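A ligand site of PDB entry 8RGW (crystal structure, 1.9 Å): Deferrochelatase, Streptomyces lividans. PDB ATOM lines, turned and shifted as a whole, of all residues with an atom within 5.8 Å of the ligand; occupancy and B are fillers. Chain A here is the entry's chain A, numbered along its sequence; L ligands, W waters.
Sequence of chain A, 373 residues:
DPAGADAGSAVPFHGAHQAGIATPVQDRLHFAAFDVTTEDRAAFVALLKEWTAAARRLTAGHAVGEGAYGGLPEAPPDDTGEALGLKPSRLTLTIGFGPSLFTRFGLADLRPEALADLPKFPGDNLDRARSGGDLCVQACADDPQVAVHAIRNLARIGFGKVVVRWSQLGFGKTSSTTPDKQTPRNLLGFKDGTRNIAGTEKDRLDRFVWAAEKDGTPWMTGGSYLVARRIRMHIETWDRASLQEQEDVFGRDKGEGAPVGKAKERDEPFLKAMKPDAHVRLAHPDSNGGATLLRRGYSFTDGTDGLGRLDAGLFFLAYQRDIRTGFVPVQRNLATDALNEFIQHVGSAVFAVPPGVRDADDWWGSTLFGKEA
The backbone NH of Thr 194 lies within hydrogen-bond range of an oxygen (O1) of the ligand, 3.2 Å away. N of Arg 195 sits at hydrogen-bond distance from O2 of the ligand (3.1 Å). A ring nitrogen (NE2) of His 279 is bound to an iron atom (FE1) of the ligand (2.1 Å). NE of Arg 195 is in salt-bridge range of O3 of the ligand. An oxygen (O1) of the ligand lies within hydrogen-bond range of the backbone NH of Gly 193 (2.6 Å). The guanidinium group (NH2) of Arg 295 lies within salt-bridge range of an oxygen (O1) of the ligand (2.9 Å).
OD1 of Asn 186 is in hydrogen-bond range of N of Leu 188. ND2 of Asn 186 lies within hydrogen-bond range of OD2 of Asp 192. The guanidinium group (NH2) of Arg 295 is in hydrogen-bond range of the backbone carbonyl oxygen (O) of Arg 195 (3.1 Å). The backbone carbonyl oxygen of Leu 293 lies close to the side-chain amide oxygen of Asn 196 (3.3 Å). The side-chain amide oxygen (OD1) of Asn 196 is in hydrogen-bond range of the backbone NH (N) of Arg 295 (2.8 Å). The backbone NH (N) of Val 280 sits at hydrogen-bond distance from the backbone carbonyl oxygen (O) of Phe 250, 3.1 Å away. O of Ile 231 sits at hydrogen-bond distance from N of Leu 314, at 2.8 Å. NH1 of Arg 295 lies within salt-bridge range of OD1 of Asp 192.
Merely in contact with the ligand: Asn 186 (3.3 Å), Phe 190 (3.7 Å), Lys 191 (3.1 Å), Asp 192 (3.6 Å), Ile 231 (3.8 Å), Met 233 (3.6 Å), Phe 250 (3.3 Å), Arg 252 (3.6 Å), Val 280 (3.6 Å), Ala 283 (3.6 Å), His 284 (3.5 Å), Pro 285 (3.2 Å), Leu 293 (3.9 Å), Leu 314 (3.98 Å), Phe 316 (3.4 Å), Phe 327 (3.3 Å), Val 330 (3.7 Å), Gln 331 (3.2 Å), Leu 334 (3.8 Å), Leu 339 (3.6 Å), Ile 343 (3.7 Å) and His 345 (3.9 Å). Hydrophobic or aromatic side chains within 4 Å of the ligand: Phe 190, Ile 231, Met 233, Phe 250, His 279, Val 280, Ala 283, His 284, Pro 285, Leu 293, Leu 314, Phe 316, Phe 327, Val 330, Leu 334, Leu 339, Ile 343 and His 345. Of the 31 residues printed, 27 come within 4 Å of the ligand. The nearest printed residue that does not touch the ligand is Leu 188 (4.1 Å).
Water W5 lies within hydrogen-bond range of O4 of the ligand (2.5 Å) and O of Arg 195 (2.8 Å). Water W1 lies within hydrogen-bond range of O2 of the ligand (2.7 Å) and NE of Arg 252 (2.8 Å). Water W2 lies within hydrogen-bond range of a ring nitrogen (NE2) of His 345 (2.7 Å) and the side-chain amide oxygen (OE1) of Gln 331 (3.1 Å).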
ATOM      1  N   ASN A 186      -1.431   0.745  24.735  1.00  0.00           N
ATOM      2  CA  ASN A 186      -0.947   0.499  23.389  1.00  0.00           C
ATOM      3  C   ASN A 186      -1.606   1.482  22.423  1.00  0.00           C
ATOM      4  O   ASN A 186      -2.421   2.327  22.799  1.00  0.00           O
ATOM      5  CB  ASN A 186      -1.192  -0.963  23.007  1.00  0.00           C
ATOM      6  CG  ASN A 186      -2.650  -1.371  23.110  1.00  0.00           C
ATOM      7  OD1 ASN A 186      -3.557  -0.599  22.766  1.00  0.00           O
ATOM      8  ND2 ASN A 186      -2.894  -2.566  23.618  1.00  0.00           N
ATOM      9  N   LEU A 188      -3.804   1.066  20.221  1.00  0.00           N
ATOM     10  CA  LEU A 188      -5.254   0.928  20.101  1.00  0.00           C
ATOM     11  C   LEU A 188      -5.994   1.658  21.205  1.00  0.00           C
ATOM     12  O   LEU A 188      -7.226   1.694  21.186  1.00  0.00           O
ATOM     13  CB  LEU A 188      -5.642  -0.554  20.092  1.00  0.00           C
ATOM     14  CG  LEU A 188      -5.032  -1.379  18.949  1.00  0.00           C
ATOM     15  CD1 LEU A 188      -5.705  -2.741  18.833  1.00  0.00           C
ATOM     16  CD2 LEU A 188      -5.111  -0.611  17.636  1.00  0.00           C
ATOM     17  N   PHE A 190      -5.914   0.987  24.536  1.00  0.00           N
ATOM     18  CA  PHE A 190      -6.271   0.180  25.691  1.00  0.00           C
ATOM     19  C   PHE A 190      -5.060  -0.016  26.603  1.00  0.00           C
ATOM     20  O   PHE A 190      -3.919  -0.095  26.140  1.00  0.00           O
ATOM     21  CB  PHE A 190      -6.806  -1.189  25.276  1.00  0.00           C
ATOM     22  CG  PHE A 190      -8.240  -1.165  24.839  1.00  0.00           C
ATOM     23  CD1 PHE A 190      -8.595  -0.629  23.615  1.00  0.00           C
ATOM     24  CD2 PHE A 190      -9.236  -1.659  25.666  1.00  0.00           C
ATOM     25  CE1 PHE A 190      -9.923  -0.606  23.222  1.00  0.00           C
ATOM     26  CE2 PHE A 190     -10.563  -1.634  25.282  1.00  0.00           C
ATOM     27  CZ  PHE A 190     -10.904  -1.099  24.048  1.00  0.00           C
ATOM     28  N   LYS A 191      -5.325  -0.074  27.900  1.00  0.00           N
ATOM     29  CA  LYS A 191      -4.296  -0.455  28.845  1.00  0.00           C
ATOM     30  C   LYS A 191      -3.787  -1.846  28.513  1.00  0.00           C
ATOM     31  O   LYS A 191      -4.570  -2.755  28.205  1.00  0.00           O
ATOM     32  CB  LYS A 191      -4.856  -0.446  30.265  1.00  0.00           C
ATOM     33  CG  LYS A 191      -5.202   0.944  30.774  1.00  0.00           C
ATOM     34  CD  LYS A 191      -5.862   0.844  32.137  1.00  0.00           C
ATOM     35  CE  LYS A 191      -6.070   2.207  32.775  1.00  0.00           C
ATOM     36  NZ  LYS A 191      -6.645   2.068  34.136  1.00  0.00           N
ATOM     37  N   ASP A 192      -2.472  -2.030  28.577  1.00  0.00           N
ATOM     38  CA  ASP A 192      -1.847  -3.270  28.144  1.00  0.00           C
ATOM     39  C   ASP A 192      -0.844  -3.679  29.215  1.00  0.00           C
ATOM     40  O   ASP A 192       0.152  -2.971  29.438  1.00  0.00           O
ATOM     41  CB  ASP A 192      -1.175  -3.104  26.781  1.00  0.00           C
ATOM     42  CG  ASP A 192      -1.016  -4.417  26.044  1.00  0.00           C
ATOM     43  OD1 ASP A 192      -1.084  -5.489  26.680  1.00  0.00           O
ATOM     44  OD2 ASP A 192      -0.835  -4.375  24.808  1.00  0.00           O
ATOM     45  N   GLY A 193      -1.106  -4.801  29.883  1.00  0.00           N
ATOM     46  CA  GLY A 193      -0.206  -5.286  30.922  1.00  0.00           C
ATOM     47  C   GLY A 193      -0.852  -5.384  32.285  1.00  0.00           C
ATOM     48  O   GLY A 193      -0.137  -5.552  33.291  1.00  0.00           O
ATOM     49  N   THR A 194      -2.184  -5.298  32.347  1.00  0.00           N
ATOM     50  CA  THR A 194      -2.869  -5.361  33.643  1.00  0.00           C
ATOM     51  C   THR A 194      -2.652  -6.698  34.327  1.00  0.00           C
ATOM     52  O   THR A 194      -2.197  -6.749  35.470  1.00  0.00           O
ATOM     53  CB  THR A 194      -4.366  -5.089  33.460  1.00  0.00           C
ATOM     54  OG1 THR A 194      -4.572  -3.742  33.018  1.00  0.00           O
ATOM     55  CG2 THR A 194      -5.110  -5.308  34.779  1.00  0.00           C
ATOM     56  N   ARG A 195      -2.958  -7.798  33.636  1.00  0.00           N
ATOM     57  CA  ARG A 195      -2.784  -9.132  34.196  1.00  0.00           C
ATOM     58  C   ARG A 195      -1.554  -9.761  33.556  1.00  0.00           C
ATOM     59  O   ARG A 195      -1.643 -10.599  32.648  1.00  0.00           O
ATOM     60  CB  ARG A 195      -4.025  -9.976  33.997  1.00  0.00           C
ATOM     61  CG  ARG A 195      -5.087  -9.715  35.052  1.00  0.00           C
ATOM     62  CD  ARG A 195      -6.336 -10.550  34.780  1.00  0.00           C
ATOM     63  NE  ARG A 195      -5.996 -11.900  34.346  1.00  0.00           N
ATOM     64  CZ  ARG A 195      -5.492 -12.837  35.139  1.00  0.00           C
ATOM     65  NH1 ARG A 195      -5.335 -12.636  36.438  1.00  0.00           N
ATOM     66  NH2 ARG A 195      -5.140 -14.004  34.617  1.00  0.00           N
ATOM     67  N   ASN A 196      -0.393  -9.339  34.030  1.00  0.00           N
ATOM     68  CA  ASN A 196       0.908  -9.875  33.650  1.00  0.00           C
ATOM     69  C   ASN A 196       1.532 -10.502  34.895  1.00  0.00           C
ATOM     70  O   ASN A 196       0.913 -10.571  35.951  1.00  0.00           O
ATOM     71  CB  ASN A 196       1.783  -8.760  33.070  1.00  0.00           C
ATOM     72  CG  ASN A 196       2.922  -9.282  32.219  1.00  0.00           C
ATOM     73  OD1 ASN A 196       2.780 -10.270  31.505  1.00  0.00           O
ATOM     74  ND2 ASN A 196       4.073  -8.612  32.300  1.00  0.00           N
ATOM     75  N   ILE A 231       4.050  -7.068  15.230  1.00  0.00           N
ATOM     76  CA  ILE A 231       2.633  -7.072  14.879  1.00  0.00           C
ATOM     77  C   ILE A 231       2.246  -5.693  14.376  1.00  0.00           C
ATOM     78  O   ILE A 231       2.302  -4.711  15.120  1.00  0.00           O
ATOM     79  CB  ILE A 231       1.752  -7.480  16.070  1.00  0.00           C
ATOM     80  CG1 ILE A 231       2.194  -8.844  16.623  1.00  0.00           C
ATOM     81  CG2 ILE A 231       0.288  -7.505  15.670  1.00  0.00           C
ATOM     82  CD1 ILE A 231       1.716  -9.130  18.029  1.00  0.00           C
ATOM     83  N   ARG A 232       1.846  -5.624  13.111  1.00  0.00           N
ATOM     84  CA  ARG A 232       1.267  -4.410  12.547  1.00  0.00           C
ATOM     85  C   ARG A 232      -0.176  -4.260  13.021  1.00  0.00           C
ATOM     86  O   ARG A 232      -0.894  -5.250  13.162  1.00  0.00           O
ATOM     87  CB  ARG A 232       1.292  -4.463  11.018  1.00  0.00           C
ATOM     88  CG  ARG A 232       0.813  -3.189  10.336  1.00  0.00           C
ATOM     89  CD  ARG A 232       0.879  -3.286   8.815  1.00  0.00           C
ATOM     90  NE  ARG A 232       2.188  -3.716   8.319  1.00  0.00           N
ATOM     91  CZ  ARG A 232       3.333  -3.117   8.603  1.00  0.00           C
ATOM     92  NH2 ARG A 232       4.465  -3.602   8.090  1.00  0.00           N
ATOM     93  N   MET A 233      -0.592  -3.027  13.279  1.00  0.00           N
ATOM     94  CA  MET A 233      -1.970  -2.716  13.619  1.00  0.00           C
ATOM     95  C   MET A 233      -2.630  -1.987  12.459  1.00  0.00           C
ATOM     96  O   MET A 233      -2.052  -1.046  11.897  1.00  0.00           O
ATOM     97  CB  MET A 233      -2.091  -1.872  14.884  1.00  0.00           C
ATOM     98  CG  MET A 233      -1.555  -2.532  16.132  1.00  0.00           C
ATOM     99  SD  MET A 233      -1.204  -1.325  17.426  1.00  0.00           S
ATOM    100  CE  MET A 233      -1.268  -2.371  18.877  1.00  0.00           C
ATOM    101  N   PHE A 250     -11.803  -6.879  23.139  1.00  0.00           N
ATOM    102  CA  PHE A 250     -10.904  -7.204  24.234  1.00  0.00           C
ATOM    103  C   PHE A 250     -11.605  -7.841  25.425  1.00  0.00           C
ATOM    104  O   PHE A 250     -11.048  -8.736  26.061  1.00  0.00           O
ATOM    105  CB  PHE A 250     -10.163  -5.940  24.680  1.00  0.00           C
ATOM    106  CG  PHE A 250      -9.053  -5.546  23.760  1.00  0.00           C
ATOM    107  CD1 PHE A 250      -7.945  -6.362  23.600  1.00  0.00           C
ATOM    108  CD2 PHE A 250      -9.126  -4.377  23.025  1.00  0.00           C
ATOM    109  CE1 PHE A 250      -6.923  -6.007  22.735  1.00  0.00           C
ATOM    110  CE2 PHE A 250      -8.112  -4.017  22.158  1.00  0.00           C
ATOM    111  CZ  PHE A 250      -7.010  -4.838  22.019  1.00  0.00           C
ATOM    112  N   ARG A 252     -12.601  -5.803  27.922  1.00  0.00           N
ATOM    113  CA  ARG A 252     -12.408  -4.790  28.937  1.00  0.00           C
ATOM    114  C   ARG A 252     -12.880  -3.468  28.370  1.00  0.00           C
ATOM    115  O   ARG A 252     -12.883  -3.269  27.146  1.00  0.00           O
ATOM    116  CB  ARG A 252     -10.934  -4.680  29.365  1.00  0.00           C
ATOM    117  CG  ARG A 252     -10.376  -5.908  30.093  1.00  0.00           C
ATOM    118  CD  ARG A 252      -8.871  -5.758  30.333  1.00  0.00           C
ATOM    119  NE  ARG A 252      -8.340  -6.792  31.223  1.00  0.00           N
ATOM    120  CZ  ARG A 252      -8.377  -6.742  32.550  1.00  0.00           C
ATOM    121  NH1 ARG A 252      -8.931  -5.721  33.189  1.00  0.00           N
ATOM    122  NH2 ARG A 252      -7.822  -7.729  33.250  1.00  0.00           N
ATOM    123  N   PRO A 269     -11.247 -10.696  35.893  1.00  0.00           N
ATOM    124  CA  PRO A 269     -12.202 -10.913  34.797  1.00  0.00           C
ATOM    125  C   PRO A 269     -13.183 -12.028  35.142  1.00  0.00           C
ATOM    126  O   PRO A 269     -12.818 -13.033  35.749  1.00  0.00           O
ATOM    127  CB  PRO A 269     -11.323 -11.291  33.603  1.00  0.00           C
ATOM    128  CG  PRO A 269      -9.931 -11.378  34.089  1.00  0.00           C
ATOM    129  CD  PRO A 269      -9.845 -10.808  35.462  1.00  0.00           C
ATOM    130  N   HIS A 279     -10.472 -11.087  23.255  1.00  0.00           N
ATOM    131  CA  HIS A 279      -9.038 -11.362  23.326  1.00  0.00           C
ATOM    132  C   HIS A 279      -8.631 -11.814  24.721  1.00  0.00           C
ATOM    133  O   HIS A 279      -7.868 -12.778  24.877  1.00  0.00           O
ATOM    134  CB  HIS A 279      -8.250 -10.134  22.898  1.00  0.00           C
ATOM    135  CG  HIS A 279      -6.764 -10.268  23.090  1.00  0.00           C
ATOM    136  ND1 HIS A 279      -5.943 -10.918  22.199  1.00  0.00           N
ATOM    137  CD2 HIS A 279      -5.948  -9.806  24.075  1.00  0.00           C
ATOM    138  CE1 HIS A 279      -4.704 -10.868  22.630  1.00  0.00           C
ATOM    139  NE2 HIS A 279      -4.673 -10.197  23.764  1.00  0.00           N
ATOM    140  N   VAL A 280      -9.115 -11.126  25.757  1.00  0.00           N
ATOM    141  CA  VAL A 280      -8.760 -11.501  27.128  1.00  0.00           C
ATOM    142  C   VAL A 280      -9.299 -12.884  27.465  1.00  0.00           C
ATOM    143  O   VAL A 280      -8.616 -13.700  28.092  1.00  0.00           O
ATOM    144  CB  VAL A 280      -9.238 -10.430  28.117  1.00  0.00           C
ATOM    145  CG1 VAL A 280      -9.057 -10.904  29.559  1.00  0.00           C
ATOM    146  CG2 VAL A 280      -8.498  -9.124  27.899  1.00  0.00           C
ATOM    147  N   ALA A 283      -7.068 -15.450  25.718  1.00  0.00           N
ATOM    148  CA  ALA A 283      -5.678 -15.466  26.153  1.00  0.00           C
ATOM    149  C   ALA A 283      -5.518 -15.726  27.644  1.00  0.00           C
ATOM    150  O   ALA A 283      -4.388 -15.984  28.088  1.00  0.00           O
ATOM    151  CB  ALA A 283      -5.011 -14.134  25.797  1.00  0.00           C
ATOM    152  N   HIS A 284      -6.606 -15.687  28.407  1.00  0.00           N
ATOM    153  CA  HIS A 284      -6.528 -15.864  29.853  1.00  0.00           C
ATOM    154  C   HIS A 284      -5.968 -17.246  30.188  1.00  0.00           C
ATOM    155  O   HIS A 284      -6.233 -18.216  29.468  1.00  0.00           O
ATOM    156  CB  HIS A 284      -7.924 -15.695  30.457  1.00  0.00           C
ATOM    157  CG  HIS A 284      -7.929 -15.523  31.948  1.00  0.00           C
ATOM    158  ND1 HIS A 284      -7.746 -16.568  32.820  1.00  0.00           N
ATOM    159  CD2 HIS A 284      -8.125 -14.419  32.717  1.00  0.00           C
ATOM    160  CE1 HIS A 284      -7.813 -16.126  34.056  1.00  0.00           C
ATOM    161  NE2 HIS A 284      -8.037 -14.825  34.025  1.00  0.00           N
ATOM    162  N   PRO A 285      -5.167 -17.372  31.251  1.00  0.00           N
ATOM    163  CA  PRO A 285      -4.629 -18.695  31.618  1.00  0.00           C
ATOM    164  C   PRO A 285      -5.703 -19.744  31.818  1.00  0.00           C
ATOM    165  O   PRO A 285      -5.488 -20.912  31.455  1.00  0.00           O
ATOM    166  CB  PRO A 285      -3.871 -18.402  32.909  1.00  0.00           C
ATOM    167  CG  PRO A 285      -3.362 -17.015  32.713  1.00  0.00           C
ATOM    168  CD  PRO A 285      -4.495 -16.295  31.997  1.00  0.00           C
ATOM    169  N   LEU A 293       2.101 -16.100  30.649  1.00  0.00           N
ATOM    170  CA  LEU A 293       3.226 -15.457  29.975  1.00  0.00           C
ATOM    171  C   LEU A 293       3.662 -14.219  30.740  1.00  0.00           C
ATOM    172  O   LEU A 293       2.876 -13.605  31.466  1.00  0.00           O
ATOM    173  CB  LEU A 293       2.859 -15.041  28.546  1.00  0.00           C
ATOM    174  CG  LEU A 293       2.287 -16.106  27.609  1.00  0.00           C
ATOM    175  CD1 LEU A 293       1.717 -15.458  26.363  1.00  0.00           C
ATOM    176  CD2 LEU A 293       3.389 -17.070  27.249  1.00  0.00           C
ATOM    177  N   ARG A 295       4.600 -10.809  29.501  1.00  0.00           N
ATOM    178  CA  ARG A 295       4.595  -9.912  28.353  1.00  0.00           C
ATOM    179  C   ARG A 295       5.434  -8.678  28.665  1.00  0.00           C
ATOM    180  O   ARG A 295       5.369  -8.141  29.765  1.00  0.00           O
ATOM    181  CB  ARG A 295       3.155  -9.526  28.023  1.00  0.00           C
ATOM    182  CG  ARG A 295       2.362 -10.663  27.374  1.00  0.00           C
ATOM    183  CD  ARG A 295       0.910 -10.302  27.169  1.00  0.00           C
ATOM    184  NE  ARG A 295       0.219 -10.160  28.444  1.00  0.00           N
ATOM    185  CZ  ARG A 295      -0.561  -9.144  28.775  1.00  0.00           C
ATOM    186  NH1 ARG A 295      -0.802  -8.150  27.940  1.00  0.00           N
ATOM    187  NH2 ARG A 295      -1.122  -9.125  29.981  1.00  0.00           N
ATOM    188  N   LEU A 314       2.892  -3.100  17.330  1.00  0.00           N
ATOM    189  CA  LEU A 314       3.328  -3.493  18.656  1.00  0.00           C
ATOM    190  C   LEU A 314       4.405  -4.553  18.491  1.00  0.00           C
ATOM    191  O   LEU A 314       4.200  -5.542  17.776  1.00  0.00           O
ATOM    192  CB  LEU A 314       2.146  -4.035  19.475  1.00  0.00           C
ATOM    193  CG  LEU A 314       2.294  -4.206  20.992  1.00  0.00           C
ATOM    194  CD1 LEU A 314       0.948  -3.990  21.672  1.00  0.00           C
ATOM    195  CD2 LEU A 314       2.852  -5.571  21.345  1.00  0.00           C
ATOM    196  N   PHE A 316       5.801  -7.347  20.085  1.00  0.00           N
ATOM    197  CA  PHE A 316       5.351  -8.203  21.184  1.00  0.00           C
ATOM    198  C   PHE A 316       6.517  -9.056  21.669  1.00  0.00           C
ATOM    199  O   PHE A 316       7.146  -9.773  20.884  1.00  0.00           O
ATOM    200  CB  PHE A 316       4.194  -9.074  20.698  1.00  0.00           C
ATOM    201  CG  PHE A 316       3.647 -10.001  21.744  1.00  0.00           C
ATOM    202  CD1 PHE A 316       2.669  -9.562  22.622  1.00  0.00           C
ATOM    203  CD2 PHE A 316       4.098 -11.305  21.842  1.00  0.00           C
ATOM    204  CE1 PHE A 316       2.147 -10.405  23.586  1.00  0.00           C
ATOM    205  CE2 PHE A 316       3.578 -12.162  22.808  1.00  0.00           C
ATOM    206  CZ  PHE A 316       2.613 -11.708  23.674  1.00  0.00           C
ATOM    207  N   PHE A 327       3.802 -19.461  24.921  1.00  0.00           N
ATOM    208  CA  PHE A 327       3.288 -18.703  23.780  1.00  0.00           C
ATOM    209  C   PHE A 327       2.506 -19.583  22.820  1.00  0.00           C
ATOM    210  O   PHE A 327       1.449 -19.174  22.314  1.00  0.00           O
ATOM    211  CB  PHE A 327       4.443 -18.014  23.050  1.00  0.00           C
ATOM    212  CG  PHE A 327       4.046 -17.325  21.781  1.00  0.00           C
ATOM    213  CD1 PHE A 327       3.551 -16.022  21.813  1.00  0.00           C
ATOM    214  CD2 PHE A 327       4.180 -17.945  20.553  1.00  0.00           C
ATOM    215  CE1 PHE A 327       3.188 -15.385  20.645  1.00  0.00           C
ATOM    216  CE2 PHE A 327       3.818 -17.308  19.385  1.00  0.00           C
ATOM    217  CZ  PHE A 327       3.318 -16.025  19.430  1.00  0.00           C
ATOM    218  N   VAL A 330      -1.167 -20.392  23.854  1.00  0.00           N
ATOM    219  CA  VAL A 330      -1.953 -19.156  23.889  1.00  0.00           C
ATOM    220  C   VAL A 330      -2.197 -18.640  22.489  1.00  0.00           C
ATOM    221  O   VAL A 330      -3.323 -18.259  22.137  1.00  0.00           O
ATOM    222  CB  VAL A 330      -1.243 -18.103  24.770  1.00  0.00           C
ATOM    223  CG1 VAL A 330      -2.044 -16.807  24.785  1.00  0.00           C
ATOM    224  CG2 VAL A 330      -1.061 -18.632  26.181  1.00  0.00           C
ATOM    225  N   GLN A 331      -1.155 -18.603  21.651  1.00  0.00           N
ATOM    226  CA  GLN A 331      -1.312 -18.100  20.286  1.00  0.00           C
ATOM    227  C   GLN A 331      -2.214 -18.997  19.456  1.00  0.00           C
ATOM    228  O   GLN A 331      -2.979 -18.513  18.624  1.00  0.00           O
ATOM    229  CB  GLN A 331       0.056 -17.949  19.622  1.00  0.00           C
ATOM    230  CG  GLN A 331       0.013 -17.389  18.201  1.00  0.00           C
ATOM    231  CD  GLN A 331      -0.626 -16.016  18.107  1.00  0.00           C
ATOM    232  OE1 GLN A 331      -0.508 -15.188  19.017  1.00  0.00           O
ATOM    233  NE2 GLN A 331      -1.317 -15.753  16.996  1.00  0.00           N
ATOM    234  N   LEU A 334      -5.676 -18.053  20.079  1.00  0.00           N
ATOM    235  CA  LEU A 334      -6.083 -16.785  19.482  1.00  0.00           C
ATOM    236  C   LEU A 334      -6.427 -16.915  18.005  1.00  0.00           C
ATOM    237  O   LEU A 334      -6.557 -15.899  17.311  1.00  0.00           O
ATOM    238  CB  LEU A 334      -4.992 -15.724  19.665  1.00  0.00           C
ATOM    239  CG  LEU A 334      -4.536 -15.420  21.098  1.00  0.00           C
ATOM    240  CD1 LEU A 334      -3.453 -14.341  21.085  1.00  0.00           C
ATOM    241  CD2 LEU A 334      -5.710 -15.008  21.965  1.00  0.00           C
ATOM    242  N   LEU A 339      -9.495  -9.783  17.793  1.00  0.00           N
ATOM    243  CA  LEU A 339      -8.430  -8.827  17.515  1.00  0.00           C
ATOM    244  C   LEU A 339      -7.740  -9.114  16.191  1.00  0.00           C
ATOM    245  O   LEU A 339      -7.115  -8.210  15.626  1.00  0.00           O
ATOM    246  CB  LEU A 339      -7.416  -8.839  18.668  1.00  0.00           C
ATOM    247  CG  LEU A 339      -6.204  -7.920  18.582  1.00  0.00           C
ATOM    248  CD1 LEU A 339      -6.647  -6.470  18.583  1.00  0.00           C
ATOM    249  CD2 LEU A 339      -5.228  -8.184  19.721  1.00  0.00           C
ATOM    250  N   ILE A 343      -4.990  -6.747  13.328  1.00  0.00           N
ATOM    251  CA  ILE A 343      -3.555  -6.920  13.504  1.00  0.00           C
ATOM    252  C   ILE A 343      -3.044  -7.919  12.486  1.00  0.00           C
ATOM    253  O   ILE A 343      -3.818  -8.660  11.858  1.00  0.00           O
ATOM    254  CB  ILE A 343      -3.201  -7.402  14.932  1.00  0.00           C
ATOM    255  CG1 ILE A 343      -3.796  -8.789  15.197  1.00  0.00           C
ATOM    256  CG2 ILE A 343      -3.637  -6.381  15.980  1.00  0.00           C
ATOM    257  CD1 ILE A 343      -3.241  -9.479  16.419  1.00  0.00           C
ATOM    258  N   HIS A 345       0.670 -10.399  12.223  1.00  0.00           N
ATOM    259  CA  HIS A 345       2.039 -10.734  12.615  1.00  0.00           C
ATOM    260  C   HIS A 345       2.924 -10.677  11.386  1.00  0.00           C
ATOM    261  O   HIS A 345       2.693 -11.401  10.406  1.00  0.00           O
ATOM    262  CB  HIS A 345       2.084 -12.123  13.251  1.00  0.00           C
ATOM    263  CG  HIS A 345       1.325 -12.219  14.540  1.00  0.00           C
ATOM    264  ND1 HIS A 345       1.916 -12.599  15.727  1.00  0.00           N
ATOM    265  CD2 HIS A 345       0.023 -11.999  14.836  1.00  0.00           C
ATOM    266  CE1 HIS A 345       1.011 -12.598  16.693  1.00  0.00           C
ATOM    267  NE2 HIS A 345      -0.140 -12.232  16.172  1.00  0.00           N
HETATM  268  C1  LIG L   1      -4.212  -9.150  27.614  1.00  0.00           C
HETATM  269  C2  LIG L   1      -3.792  -6.113  23.847  1.00  0.00           C
HETATM  270  C3  LIG L   1      -1.312  -9.495  21.422  1.00  0.00           C
HETATM  271  C4  LIG L   1      -1.504 -12.431  25.271  1.00  0.00           C
HETATM  272  C5  LIG L   1      -4.347  -8.045  26.806  1.00  0.00           C
HETATM  273  C6  LIG L   1      -5.089  -6.832  27.118  1.00  0.00           C
HETATM  274  C7  LIG L   1      -4.970  -6.005  26.065  1.00  0.00           C
HETATM  275  C8  LIG L   1      -4.143  -6.650  25.062  1.00  0.00           C
HETATM  276  C9  LIG L   1      -5.592  -4.600  25.927  1.00  0.00           C
HETATM  277  C10 LIG L   1      -5.880  -6.582  28.425  1.00  0.00           C
HETATM  278  C11 LIG L   1      -5.014  -5.966  29.518  1.00  0.00           C
HETATM  279  C12 LIG L   1      -3.963  -6.918  30.025  1.00  0.00           C
HETATM  280  O1  LIG L   1      -2.792  -6.799  29.604  1.00  0.00           O
HETATM  281  O2  LIG L   1      -4.294  -7.798  30.868  1.00  0.00           O
HETATM  282  C13 LIG L   1      -3.073  -6.748  22.860  1.00  0.00           C
HETATM  283  C14 LIG L   1      -2.668  -6.186  21.582  1.00  0.00           C
HETATM  284  C15 LIG L   1      -1.982  -7.122  20.913  1.00  0.00           C
HETATM  285  C16 LIG L   1      -1.923  -8.305  21.751  1.00  0.00           C
HETATM  286  C17 LIG L   1      -3.022  -4.735  21.140  1.00  0.00           C
HETATM  287  C18 LIG L   1      -1.323  -7.066  19.506  1.00  0.00           C
HETATM  288  C19 LIG L   1      -1.249  -5.977  18.736  1.00  0.00           C
HETATM  289  C20 LIG L   1      -1.172 -10.591  22.239  1.00  0.00           C
HETATM  290  C21 LIG L   1      -0.565 -11.860  21.871  1.00  0.00           C
HETATM  291  C22 LIG L   1      -0.607 -12.666  22.943  1.00  0.00           C
HETATM  292  C23 LIG L   1      -1.260 -11.945  24.010  1.00  0.00           C
HETATM  293  C24 LIG L   1       0.032 -12.147  20.484  1.00  0.00           C
HETATM  294  C25 LIG L   1      -0.128 -14.131  23.137  1.00  0.00           C
HETATM  295  C26 LIG L   1       0.236 -14.938  22.136  1.00  0.00           C
HETATM  296  C27 LIG L   1      -2.213 -11.766  26.254  1.00  0.00           C
HETATM  297  C28 LIG L   1      -2.381 -12.234  27.615  1.00  0.00           C
HETATM  298  C29 LIG L   1      -3.127 -11.331  28.257  1.00  0.00           C
HETATM  299  C30 LIG L   1      -3.462 -10.264  27.328  1.00  0.00           C
HETATM  300  C31 LIG L   1      -1.805 -13.532  28.201  1.00  0.00           C
HETATM  301  C32 LIG L   1      -3.559 -11.426  29.737  1.00  0.00           C
HETATM  302  C33 LIG L   1      -4.948 -12.035  29.791  1.00  0.00           C
HETATM  303  C34 LIG L   1      -5.299 -12.313  31.230  1.00  0.00           C
HETATM  304  O3  LIG L   1      -6.251 -11.673  31.745  1.00  0.00           O
HETATM  305  O4  LIG L   1      -4.615 -13.142  31.860  1.00  0.00           O
HETATM  306  N1  LIG L   1      -3.788  -7.891  25.553  1.00  0.00           N
HETATM  307  N2  LIG L   1      -2.594  -8.039  22.927  1.00  0.00           N
HETATM  308  N3  LIG L   1      -1.590 -10.680  23.556  1.00  0.00           N
HETATM  309  N4  LIG L   1      -2.878 -10.570  26.115  1.00  0.00           N
HETATM  310 FE1  LIG L   1      -2.843  -9.360  24.486  1.00  0.00          FE
HETATM  311  O   HOH W   1      -6.690  -9.040  31.001  1.00  0.00           O
HETATM  312  O   HOH W   2      -2.066 -12.706  17.972  1.00  0.00           O
HETATM  313  O   HOH W   3      -1.826 -16.633  29.166  1.00  0.00           O
HETATM  314  O   HOH W   4      -0.353 -14.816  30.691  1.00  0.00           O
HETATM  315  O   HOH W   5      -2.219 -13.333  32.541  1.00  0.00           O
